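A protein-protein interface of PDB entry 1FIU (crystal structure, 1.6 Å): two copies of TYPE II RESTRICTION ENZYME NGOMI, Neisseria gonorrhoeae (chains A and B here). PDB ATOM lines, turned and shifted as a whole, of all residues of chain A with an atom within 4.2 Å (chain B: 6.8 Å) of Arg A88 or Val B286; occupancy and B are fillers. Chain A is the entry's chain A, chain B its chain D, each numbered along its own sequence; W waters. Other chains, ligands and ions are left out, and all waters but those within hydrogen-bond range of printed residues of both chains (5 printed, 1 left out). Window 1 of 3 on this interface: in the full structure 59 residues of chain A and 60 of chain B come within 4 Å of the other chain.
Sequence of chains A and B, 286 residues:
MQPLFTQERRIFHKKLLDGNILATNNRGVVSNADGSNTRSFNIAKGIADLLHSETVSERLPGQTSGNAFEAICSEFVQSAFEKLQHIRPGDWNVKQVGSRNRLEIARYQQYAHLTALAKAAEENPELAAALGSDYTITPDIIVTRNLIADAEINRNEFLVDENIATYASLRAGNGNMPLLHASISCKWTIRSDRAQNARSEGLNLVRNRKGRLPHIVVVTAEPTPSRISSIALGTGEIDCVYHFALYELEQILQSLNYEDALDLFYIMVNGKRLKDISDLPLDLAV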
ATOM      1  N   LEU A  84       5.533   7.283   0.349  1.00  0.00           N
ATOM      2  CA  LEU A  84       6.867   7.854   0.466  1.00  0.00           C
ATOM      3  C   LEU A  84       7.654   7.856  -0.858  1.00  0.00           C
ATOM      4  O   LEU A  84       8.879   7.979  -0.867  1.00  0.00           O
ATOM      5  CB  LEU A  84       7.639   7.094   1.558  1.00  0.00           C
ATOM      6  CG  LEU A  84       7.040   7.211   2.977  1.00  0.00           C
ATOM      7  CD1 LEU A  84       7.809   6.315   3.941  1.00  0.00           C
ATOM      8  CD2 LEU A  84       7.081   8.671   3.442  1.00  0.00           C
ATOM      9  N   GLN A  85       6.949   7.748  -1.973  1.00  0.00           N
ATOM     10  CA  GLN A  85       7.612   7.727  -3.280  1.00  0.00           C
ATOM     11  C   GLN A  85       8.519   8.947  -3.552  1.00  0.00           C
ATOM     12  O   GLN A  85       9.482   8.845  -4.315  1.00  0.00           O
ATOM     13  CB  GLN A  85       6.566   7.583  -4.390  1.00  0.00           C
ATOM     14  CG  GLN A  85       7.153   7.631  -5.793  1.00  0.00           C
ATOM     15  CD  GLN A  85       7.613   6.264  -6.299  1.00  0.00           C
ATOM     16  OE1 GLN A  85       8.275   6.170  -7.335  1.00  0.00           O
ATOM     17  NE2 GLN A  85       7.244   5.204  -5.581  1.00  0.00           N
ATOM     18  N   HIS A  86       8.225  10.097  -2.954  1.00  0.00           N
ATOM     19  CA  HIS A  86       9.060  11.282  -3.167  1.00  0.00           C
ATOM     20  C   HIS A  86      10.373  11.247  -2.393  1.00  0.00           C
ATOM     21  O   HIS A  86      11.312  11.966  -2.736  1.00  0.00           O
ATOM     22  CB  HIS A  86       8.290  12.575  -2.821  1.00  0.00           C
ATOM     23  CG  HIS A  86       7.841  12.654  -1.398  1.00  0.00           C
ATOM     24  ND1 HIS A  86       6.992  11.725  -0.836  1.00  0.00           N
ATOM     25  CD2 HIS A  86       8.122  13.550  -0.421  1.00  0.00           C
ATOM     26  CE1 HIS A  86       6.768  12.042   0.426  1.00  0.00           C
ATOM     27  NE2 HIS A  86       7.440  13.146   0.703  1.00  0.00           N
ATOM     28  N   ILE A  87      10.452  10.443  -1.336  1.00  0.00           N
ATOM     29  CA  ILE A  87      11.713  10.365  -0.615  1.00  0.00           C
ATOM     30  C   ILE A  87      12.444   9.051  -0.913  1.00  0.00           C
ATOM     31  O   ILE A  87      13.631   8.920  -0.605  1.00  0.00           O
ATOM     32  CB  ILE A  87      11.554  10.530   0.914  1.00  0.00           C
ATOM     33  CG1 ILE A  87      10.670   9.431   1.476  1.00  0.00           C
ATOM     34  CG2 ILE A  87      11.003  11.944   1.236  1.00  0.00           C
ATOM     35  CD1 ILE A  87      10.610   9.449   3.010  1.00  0.00           C
ATOM     36  N   ARG A  88      11.736   8.090  -1.517  1.00  0.00           N
ATOM     37  CA  ARG A  88      12.325   6.793  -1.884  1.00  0.00           C
ATOM     38  C   ARG A  88      11.551   6.226  -3.081  1.00  0.00           C
ATOM     39  O   ARG A  88      10.774   5.274  -2.981  1.00  0.00           O
ATOM     40  CB  ARG A  88      12.279   5.809  -0.701  1.00  0.00           C
ATOM     41  CG  ARG A  88      13.266   4.617  -0.837  1.00  0.00           C
ATOM     42  CD  ARG A  88      14.747   5.050  -0.825  1.00  0.00           C
ATOM     43  NE  ARG A  88      15.645   3.936  -0.482  1.00  0.00           N
ATOM     44  CZ  ARG A  88      16.125   3.027  -1.339  1.00  0.00           C
ATOM     45  NH1 ARG A  88      15.810   3.084  -2.638  1.00  0.00           N
ATOM     46  NH2 ARG A  88      16.902   2.045  -0.891  1.00  0.00           N
ATOM     47  N   PRO A  89      11.764   6.830  -4.244  1.00  0.00           N
ATOM     48  CA  PRO A  89      11.094   6.408  -5.469  1.00  0.00           C
ATOM     49  C   PRO A  89      11.444   5.001  -5.933  1.00  0.00           C
ATOM     50  O   PRO A  89      12.509   4.470  -5.601  1.00  0.00           O
ATOM     51  CB  PRO A  89      11.511   7.483  -6.476  1.00  0.00           C
ATOM     52  CG  PRO A  89      12.811   7.971  -5.975  1.00  0.00           C
ATOM     53  CD  PRO A  89      12.612   8.015  -4.473  1.00  0.00           C
ATOM     54  N   GLY A  90      10.526   4.386  -6.681  1.00  0.00           N
ATOM     55  CA  GLY A  90      10.791   3.051  -7.198  1.00  0.00           C
ATOM     56  C   GLY A  90       9.508   2.311  -7.505  1.00  0.00           C
ATOM     57  O   GLY A  90       8.426   2.760  -7.111  1.00  0.00           O
ATOM     58  N   TRP A  92       7.888  -0.511  -6.345  1.00  0.00           N
ATOM     59  CA  TRP A  92       7.967  -1.418  -5.191  1.00  0.00           C
ATOM     60  C   TRP A  92       6.858  -2.442  -5.069  1.00  0.00           C
ATOM     61  O   TRP A  92       5.721  -2.171  -5.436  1.00  0.00           O
ATOM     62  CB  TRP A  92       7.981  -0.592  -3.894  1.00  0.00           C
ATOM     63  CG  TRP A  92       9.002   0.507  -3.846  1.00  0.00           C
ATOM     64  CD1 TRP A  92       8.794   1.833  -4.098  1.00  0.00           C
ATOM     65  CD2 TRP A  92      10.395   0.368  -3.530  1.00  0.00           C
ATOM     66  NE1 TRP A  92       9.975   2.533  -3.954  1.00  0.00           N
ATOM     67  CE2 TRP A  92      10.973   1.661  -3.612  1.00  0.00           C
ATOM     68  CE3 TRP A  92      11.211  -0.723  -3.183  1.00  0.00           C
ATOM     69  CZ2 TRP A  92      12.332   1.897  -3.365  1.00  0.00           C
ATOM     70  CZ3 TRP A  92      12.564  -0.489  -2.932  1.00  0.00           C
ATOM     71  CH2 TRP A  92      13.112   0.812  -3.027  1.00  0.00           C
ATOM     72  N   ARG A 145      12.240  -4.299  -5.247  1.00  0.00           N
ATOM     73  CA  ARG A 145      12.291  -3.160  -6.176  1.00  0.00           C
ATOM     74  C   ARG A 145      12.501  -3.699  -7.586  1.00  0.00           C
ATOM     75  O   ARG A 145      13.454  -4.422  -7.836  1.00  0.00           O
ATOM     76  CB  ARG A 145      13.465  -2.221  -5.852  1.00  0.00           C
ATOM     77  CG  ARG A 145      13.364  -0.879  -6.591  1.00  0.00           C
ATOM     78  CD  ARG A 145      14.539   0.023  -6.332  1.00  0.00           C
ATOM     79  NE  ARG A 145      14.404   1.277  -7.072  1.00  0.00           N
ATOM     80  CZ  ARG A 145      15.197   2.329  -6.912  1.00  0.00           C
ATOM     81  NH1 ARG A 145      16.194   2.283  -6.031  1.00  0.00           N
ATOM     82  NH2 ARG A 145      14.996   3.438  -7.629  1.00  0.00           N
ATOM     83  N   LEU A 170      20.519  -1.894 -11.000  1.00  0.00           N
ATOM     84  CA  LEU A 170      19.199  -1.360 -11.331  1.00  0.00           C
ATOM     85  C   LEU A 170      18.817  -1.468 -12.774  1.00  0.00           C
ATOM     86  O   LEU A 170      17.643  -1.272 -13.097  1.00  0.00           O
ATOM     87  CB  LEU A 170      19.101   0.107 -10.956  1.00  0.00           C
ATOM     88  CG  LEU A 170      18.970   0.350  -9.462  1.00  0.00           C
ATOM     89  CD1 LEU A 170      19.201   1.833  -9.149  1.00  0.00           C
ATOM     90  CD2 LEU A 170      17.543  -0.061  -9.032  1.00  0.00           C
ATOM     91  N   LEU A 179      15.368  -6.516  -7.175  1.00  0.00           N
ATOM     92  CA  LEU A 179      16.214  -6.413  -5.981  1.00  0.00           C
ATOM     93  C   LEU A 179      15.402  -6.627  -4.704  1.00  0.00           C
ATOM     94  O   LEU A 179      14.266  -6.174  -4.597  1.00  0.00           O
ATOM     95  CB  LEU A 179      16.854  -5.022  -5.932  1.00  0.00           C
ATOM     96  CG  LEU A 179      17.932  -4.769  -7.007  1.00  0.00           C
ATOM     97  CD1 LEU A 179      18.007  -3.280  -7.354  1.00  0.00           C
ATOM     98  CD2 LEU A 179      19.286  -5.281  -6.475  1.00  0.00           C
ATOM     99  N   HIS A 181      14.583  -5.576  -1.238  1.00  0.00           N
ATOM    100  CA  HIS A 181      14.752  -4.347  -0.472  1.00  0.00           C
ATOM    101  C   HIS A 181      14.711  -4.621   1.027  1.00  0.00           C
ATOM    102  O   HIS A 181      15.483  -4.031   1.793  1.00  0.00           O
ATOM    103  CB  HIS A 181      13.635  -3.353  -0.823  1.00  0.00           C
ATOM    104  CG  HIS A 181      13.807  -2.014  -0.182  1.00  0.00           C
ATOM    105  ND1 HIS A 181      12.918  -1.497   0.740  1.00  0.00           N
ATOM    106  CD2 HIS A 181      14.786  -1.096  -0.328  1.00  0.00           C
ATOM    107  CE1 HIS A 181      13.349  -0.308   1.127  1.00  0.00           C
ATOM    108  NE2 HIS A 181      14.474  -0.042   0.491  1.00  0.00           N
ATOM    109  N   ALA A 285      12.651   3.799   4.017  1.00  0.00           N
ATOM    110  CA  ALA A 285      12.963   4.800   2.993  1.00  0.00           C
ATOM    111  C   ALA A 285      14.384   5.379   3.092  1.00  0.00           C
ATOM    112  O   ALA A 285      14.728   6.283   2.324  1.00  0.00           O
ATOM    113  CB  ALA A 285      11.942   5.948   3.071  1.00  0.00           C
ATOM    114  N   VAL A 286      15.223   4.878   4.003  1.00  0.00           N
ATOM    115  CA  VAL A 286      16.567   5.458   4.144  1.00  0.00           C
ATOM    116  C   VAL A 286      17.447   5.283   2.890  1.00  0.00           C
ATOM    117  O   VAL A 286      18.302   6.182   2.603  1.00  0.00           O
ATOM    118  CB  VAL A 286      17.333   4.865   5.353  1.00  0.00           C
ATOM    119  CG1 VAL A 286      16.588   5.162   6.664  1.00  0.00           C
ATOM    120  CG2 VAL A 286      17.522   3.386   5.150  1.00  0.00           C
ATOM    121  OXT VAL A 286      17.280   4.229   2.226  1.00  0.00           O
ATOM    122  N   PHE B  81      27.060  10.408  -8.719  1.00  0.00           N
ATOM    123  CA  PHE B  81      25.902  10.130  -7.886  1.00  0.00           C
ATOM    124  C   PHE B  81      24.953  11.324  -7.784  1.00  0.00           C
ATOM    125  O   PHE B  81      23.748  11.148  -7.614  1.00  0.00           O
ATOM    126  CB  PHE B  81      26.382   9.688  -6.486  1.00  0.00           C
ATOM    127  CG  PHE B  81      25.282   9.159  -5.608  1.00  0.00           C
ATOM    128  CD1 PHE B  81      24.557   8.061  -5.998  1.00  0.00           C
ATOM    129  CD2 PHE B  81      24.982   9.770  -4.403  1.00  0.00           C
ATOM    130  CE1 PHE B  81      23.535   7.550  -5.194  1.00  0.00           C
ATOM    131  CE2 PHE B  81      23.960   9.274  -3.584  1.00  0.00           C
ATOM    132  CZ  PHE B  81      23.240   8.180  -3.980  1.00  0.00           C
ATOM    133  N   ILE B  87      16.379   9.198  -8.872  1.00  0.00           N
ATOM    134  CA  ILE B  87      16.339   7.754  -8.614  1.00  0.00           C
ATOM    135  C   ILE B  87      16.591   7.468  -7.123  1.00  0.00           C
ATOM    136  O   ILE B  87      16.142   6.447  -6.593  1.00  0.00           O
ATOM    137  CB  ILE B  87      17.465   7.010  -9.443  1.00  0.00           C
ATOM    138  CG1 ILE B  87      17.201   7.208 -10.939  1.00  0.00           C
ATOM    139  CG2 ILE B  87      17.521   5.517  -9.101  1.00  0.00           C
ATOM    140  CD1 ILE B  87      15.809   6.891 -11.324  1.00  0.00           C
ATOM    141  N   ARG B  88      17.320   8.373  -6.463  1.00  0.00           N
ATOM    142  CA  ARG B  88      17.676   8.206  -5.035  1.00  0.00           C
ATOM    143  C   ARG B  88      17.852   9.602  -4.466  1.00  0.00           C
ATOM    144  O   ARG B  88      18.984  10.099  -4.295  1.00  0.00           O
ATOM    145  CB  ARG B  88      18.987   7.397  -4.911  1.00  0.00           C
ATOM    146  CG  ARG B  88      19.272   6.831  -3.524  1.00  0.00           C
ATOM    147  CD  ARG B  88      18.264   5.723  -3.199  1.00  0.00           C
ATOM    148  NE  ARG B  88      18.736   4.819  -2.146  1.00  0.00           N
ATOM    149  CZ  ARG B  88      18.688   5.085  -0.838  1.00  0.00           C
ATOM    150  NH1 ARG B  88      18.169   6.238  -0.405  1.00  0.00           N
ATOM    151  NH2 ARG B  88      19.201   4.224   0.034  1.00  0.00           N
ATOM    152  N   PRO B  89      16.724  10.273  -4.171  1.00  0.00           N
ATOM    153  CA  PRO B  89      16.793  11.633  -3.630  1.00  0.00           C
ATOM    154  C   PRO B  89      17.330  11.721  -2.213  1.00  0.00           C
ATOM    155  O   PRO B  89      17.323  10.729  -1.453  1.00  0.00           O
ATOM    156  CB  PRO B  89      15.344  12.131  -3.745  1.00  0.00           C
ATOM    157  CG  PRO B  89      14.520  10.866  -3.678  1.00  0.00           C
ATOM    158  CD  PRO B  89      15.338   9.881  -4.485  1.00  0.00           C
ATOM    159  N   ARG B 145      23.880  10.654   4.370  1.00  0.00           N
ATOM    160  CA  ARG B 145      22.610  11.302   4.025  1.00  0.00           C
ATOM    161  C   ARG B 145      22.156  12.168   5.199  1.00  0.00           C
ATOM    162  O   ARG B 145      22.059  11.682   6.327  1.00  0.00           O
ATOM    163  CB  ARG B 145      21.513  10.258   3.767  1.00  0.00           C
ATOM    164  CG  ARG B 145      20.217  10.856   3.204  1.00  0.00           C
ATOM    165  CD  ARG B 145      19.109   9.831   3.070  1.00  0.00           C
ATOM    166  NE  ARG B 145      17.935  10.450   2.463  1.00  0.00           N
ATOM    167  CZ  ARG B 145      16.890   9.792   1.983  1.00  0.00           C
ATOM    168  NH1 ARG B 145      16.861   8.472   2.022  1.00  0.00           N
ATOM    169  NH2 ARG B 145      15.850  10.463   1.487  1.00  0.00           N
ATOM    170  N   HIS B 181      25.547   6.097   4.484  1.00  0.00           N
ATOM    171  CA  HIS B 181      25.010   5.429   3.295  1.00  0.00           C
ATOM    172  C   HIS B 181      25.969   4.374   2.714  1.00  0.00           C
ATOM    173  O   HIS B 181      25.544   3.273   2.316  1.00  0.00           O
ATOM    174  CB  HIS B 181      24.697   6.494   2.227  1.00  0.00           C
ATOM    175  CG  HIS B 181      24.084   5.928   0.973  1.00  0.00           C
ATOM    176  ND1 HIS B 181      22.851   5.320   0.965  1.00  0.00           N
ATOM    177  CD2 HIS B 181      24.547   5.881  -0.301  1.00  0.00           C
ATOM    178  CE1 HIS B 181      22.569   4.926  -0.270  1.00  0.00           C
ATOM    179  NE2 HIS B 181      23.579   5.258  -1.055  1.00  0.00           N
ATOM    180  N   ARG B 212      19.833  -0.144   8.871  1.00  0.00           N
ATOM    181  CA  ARG B 212      20.274  -0.842   7.648  1.00  0.00           C
ATOM    182  C   ARG B 212      21.786  -0.728   7.437  1.00  0.00           C
ATOM    183  O   ARG B 212      22.383   0.329   7.650  1.00  0.00           O
ATOM    184  CB  ARG B 212      19.541  -0.315   6.396  1.00  0.00           C
ATOM    185  CG  ARG B 212      19.793  -1.199   5.134  1.00  0.00           C
ATOM    186  CD  ARG B 212      19.068  -0.744   3.880  1.00  0.00           C
ATOM    187  NE  ARG B 212      19.351  -1.704   2.804  1.00  0.00           N
ATOM    188  CZ  ARG B 212      18.948  -1.600   1.536  1.00  0.00           C
ATOM    189  NH1 ARG B 212      18.220  -0.560   1.131  1.00  0.00           N
ATOM    190  NH2 ARG B 212      19.290  -2.547   0.664  1.00  0.00           N
ATOM    191  N   HIS B 215      26.157   0.507   2.268  1.00  0.00           N
ATOM    192  CA  HIS B 215      26.802  -0.156   1.133  1.00  0.00           C
ATOM    193  C   HIS B 215      28.243  -0.381   1.630  1.00  0.00           C
ATOM    194  O   HIS B 215      28.811   0.493   2.302  1.00  0.00           O
ATOM    195  CB  HIS B 215      26.866   0.804  -0.044  1.00  0.00           C
ATOM    196  CG  HIS B 215      25.583   0.906  -0.793  1.00  0.00           C
ATOM    197  ND1 HIS B 215      24.629   1.880  -0.551  1.00  0.00           N
ATOM    198  CD2 HIS B 215      25.097   0.138  -1.787  1.00  0.00           C
ATOM    199  CE1 HIS B 215      23.608   1.698  -1.375  1.00  0.00           C
ATOM    200  NE2 HIS B 215      23.869   0.645  -2.133  1.00  0.00           N
ATOM    201  N   PRO B 281      28.213   4.373  -9.049  1.00  0.00           N
ATOM    202  CA  PRO B 281      27.198   5.403  -8.733  1.00  0.00           C
ATOM    203  C   PRO B 281      25.759   4.837  -8.787  1.00  0.00           C
ATOM    204  O   PRO B 281      24.942   5.072  -7.888  1.00  0.00           O
ATOM    205  CB  PRO B 281      27.446   6.481  -9.795  1.00  0.00           C
ATOM    206  CG  PRO B 281      28.960   6.340 -10.083  1.00  0.00           C
ATOM    207  CD  PRO B 281      29.122   4.818 -10.126  1.00  0.00           C
ATOM    208  N   LEU B 282      25.429   4.099  -9.842  1.00  0.00           N
ATOM    209  CA  LEU B 282      24.096   3.502  -9.916  1.00  0.00           C
ATOM    210  C   LEU B 282      23.864   2.441  -8.837  1.00  0.00           C
ATOM    211  O   LEU B 282      22.756   2.326  -8.316  1.00  0.00           O
ATOM    212  CB  LEU B 282      23.842   2.888 -11.324  1.00  0.00           C
ATOM    213  CG  LEU B 282      23.296   3.902 -12.332  1.00  0.00           C
ATOM    214  CD1 LEU B 282      23.490   3.329 -13.755  1.00  0.00           C
ATOM    215  CD2 LEU B 282      21.801   4.190 -12.049  1.00  0.00           C
ATOM    216  N   ASP B 283      24.897   1.677  -8.476  1.00  0.00           N
ATOM    217  CA  ASP B 283      24.721   0.671  -7.427  1.00  0.00           C
ATOM    218  C   ASP B 283      24.482   1.350  -6.067  1.00  0.00           C
ATOM    219  O   ASP B 283      23.874   0.742  -5.179  1.00  0.00           O
ATOM    220  CB  ASP B 283      25.921  -0.274  -7.362  1.00  0.00           C
ATOM    221  CG  ASP B 283      25.859  -1.345  -8.442  1.00  0.00           C
ATOM    222  OD1 ASP B 283      24.852  -1.360  -9.191  1.00  0.00           O
ATOM    223  OD2 ASP B 283      26.786  -2.175  -8.528  1.00  0.00           O
ATOM    224  N   LEU B 284      24.951   2.584  -5.913  1.00  0.00           N
ATOM    225  CA  LEU B 284      24.714   3.336  -4.664  1.00  0.00           C
ATOM    226  C   LEU B 284      23.284   3.904  -4.640  1.00  0.00           C
ATOM    227  O   LEU B 284      22.854   4.508  -3.649  1.00  0.00           O
ATOM    228  CB  LEU B 284      25.705   4.494  -4.540  1.00  0.00           C
ATOM    229  CG  LEU B 284      27.159   4.076  -4.323  1.00  0.00           C
ATOM    230  CD1 LEU B 284      28.051   5.320  -4.233  1.00  0.00           C
ATOM    231  CD2 LEU B 284      27.254   3.294  -3.012  1.00  0.00           C
ATOM    232  N   ALA B 285      22.538   3.702  -5.723  1.00  0.00           N
ATOM    233  CA  ALA B 285      21.173   4.225  -5.814  1.00  0.00           C
ATOM    234  C   ALA B 285      20.074   3.189  -5.595  1.00  0.00           C
ATOM    235  O   ALA B 285      18.893   3.510  -5.705  1.00  0.00           O
ATOM    236  CB  ALA B 285      20.969   4.927  -7.193  1.00  0.00           C
ATOM    237  N   VAL B 286      20.439   1.953  -5.260  1.00  0.00           N
ATOM    238  CA  VAL B 286      19.410   0.914  -5.079  1.00  0.00           C
ATOM    239  C   VAL B 286      18.501   1.233  -3.884  1.00  0.00           C
ATOM    240  O   VAL B 286      17.316   0.870  -3.937  1.00  0.00           O
ATOM    241  CB  VAL B 286      20.032  -0.482  -4.873  1.00  0.00           C
ATOM    242  CG1 VAL B 286      20.839  -0.900  -6.113  1.00  0.00           C
ATOM    243  CG2 VAL B 286      20.909  -0.459  -3.649  1.00  0.00           C
ATOM    244  OXT VAL B 286      18.999   1.830  -2.903  1.00  0.00           O
HETATM  245  O   HOH W   1      16.327   8.232  -1.668  1.00  0.00           O
HETATM  246  O   HOH W   2      14.784   5.289  -4.260  1.00  0.00           O
HETATM  247  O   HOH W   3      16.831   1.723   2.033  1.00  0.00           O
HETATM  248  O   HOH W   4      20.800   4.798   2.780  1.00  0.00           O
HETATM  249  O   HOH W   5      22.405  -0.083  -9.860  1.00  0.00           O
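The guanidinium group of Arg B145 is in hydrogen-bond range of the backbone carbonyl oxygen of Ile A87, 3.4 Å away.
NH2 of Arg A88 lies within salt-bridge range of OXT of Val B286, 2.9 Å away.
The backbone carbonyl oxygen of Ile B87 sits at hydrogen-bond distance from the guanidinium group of Arg A145 (3.4 Å).
NH1 of Arg A145 is in hydrogen-bond range of O of Ala B285 (3.0 Å).
The guanidinium group (NH1) of Arg A145 is in salt-bridge range of the chain-end carboxylate (O) of Val B286 (2.8 Å).
The backbone carbonyl oxygen of Ala A285 lies within hydrogen-bond range of the guanidinium group of Arg B145 (3.1 Å).
The chain-end carboxylate (OXT) of Val A286 is in salt-bridge range of the guanidinium group (NH2) of Arg B88 (2.9 Å).
The chain-end carboxylate (O) of Val A286 lies within salt-bridge range of the guanidinium group (NH1) of Arg B145.
NH2 of Arg A88 lies close to NH2 of Arg B88 (3.3 Å).
Arg A88 touches just these residues of chain B: Arg B88, Arg B212 and Val B286.
Of chain A, only Arg A88 (2.9 Å), Arg A145 (2.8 Å) and Leu A179 (3.9 Å) come within 4 Å of Val B286.
Of the printed residues of chain A, Leu B282 touches Leu A170.
Printed residues of chain A within 4 Å of Arg B212: Arg A88 (3.6 Å) and His A181 (3.8 Å).
Printed residues of chain B within 4 Å of Ile A87: Pro B89 and Arg B145.
The nearest residue of chain B that does not touch Arg A88 is Ala B285 (4.4 Å).
The nearest printed residue of chain A that does not touch Ala B285 is Arg A88 (4.4 Å).
Ile A87 touches Pro B89, and with the chains exchanged Pro A89 touches Ile B87.
Ile A87 touches Arg B145, and with the chains exchanged Arg A145 touches Ile B87.
Arg A88 touches its own counterpart, Arg B88.
Pro B89 touches its own counterpart, Pro A89.
Hydrophobic or aromatic side chains of chain B within 4 Å of the printed part of chain A: Ile B87, Pro B89 and Val B286.
Among the printed residues, 18 pairs touch across the chains.
Among the printed residues, no Asp or Glu carboxylate lies within 4 Å of a Lys or Arg side-chain nitrogen of the other chain.
Among the printed residues, pairs that only touch across the chains: His A86 with Pro B89, Ile A87 with Pro B89, Arg A88 with Arg B212, Pro A89 with Ile B87, Pro A89 with Pro B89, Leu A170 with Leu B282, Leu A170 with Ala B285, Leu A179 with Val B286 and His A181 with Arg B212.
NE1 of Trp A92 sits at hydrogen-bond distance from O of Arg A88.
A ring nitrogen (NE2) of His A181 sits at hydrogen-bond distance from the guanidinium group of Arg A88, at 3.5 Å.
The guanidinium group (NH2) of Arg A145 lies within hydrogen-bond range of the backbone carbonyl oxygen (O) of Pro A89 (3.4 Å).
The backbone NH of Arg A145 lies within hydrogen-bond range of the backbone carbonyl oxygen of Leu A179 (2.8 Å).
The guanidinium group of Arg B88 is in salt-bridge range of the chain-end carboxylate of Val B286, at 3.1 Å.
NH2 of Arg B145 is in hydrogen-bond range of O of Pro B89, 3.3 Å away.
Water W3 lies within hydrogen-bond range of the chain-end carboxylate (OXT) of Val A286 (2.6 Å), the guanidinium group (NH1) of Arg B212 (2.8 Å), the guanidinium group (NH2) of Arg A88 (2.9 Å) and a ring nitrogen (NE2) of His A181 (3.3 Å).
Water W1 lies within hydrogen-bond range of the backbone carbonyl oxygen (O) of Pro B89, the backbone carbonyl oxygen (O) of Ile A87 and the guanidinium group (NH1) of Arg B88.
Water W2 lies within hydrogen-bond range of O of Pro A89 (2.8 Å), NH1 of Arg A88 (2.9 Å) and O of Ile B87 (2.9 Å).
Water W4 lies within hydrogen-bond range of a ring nitrogen (ND1) of His B181 (2.8 Å), the chain-end carboxylate (O) of Val A286 (2.9 Å) and the guanidinium group (NH2) of Arg B88 (3.2 Å).
Water W5 lies within hydrogen-bond range of OD1 of Asp B283 (2.8 Å), N of Leu A170 (2.9 Å) and O of Leu B282 (2.9 Å).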
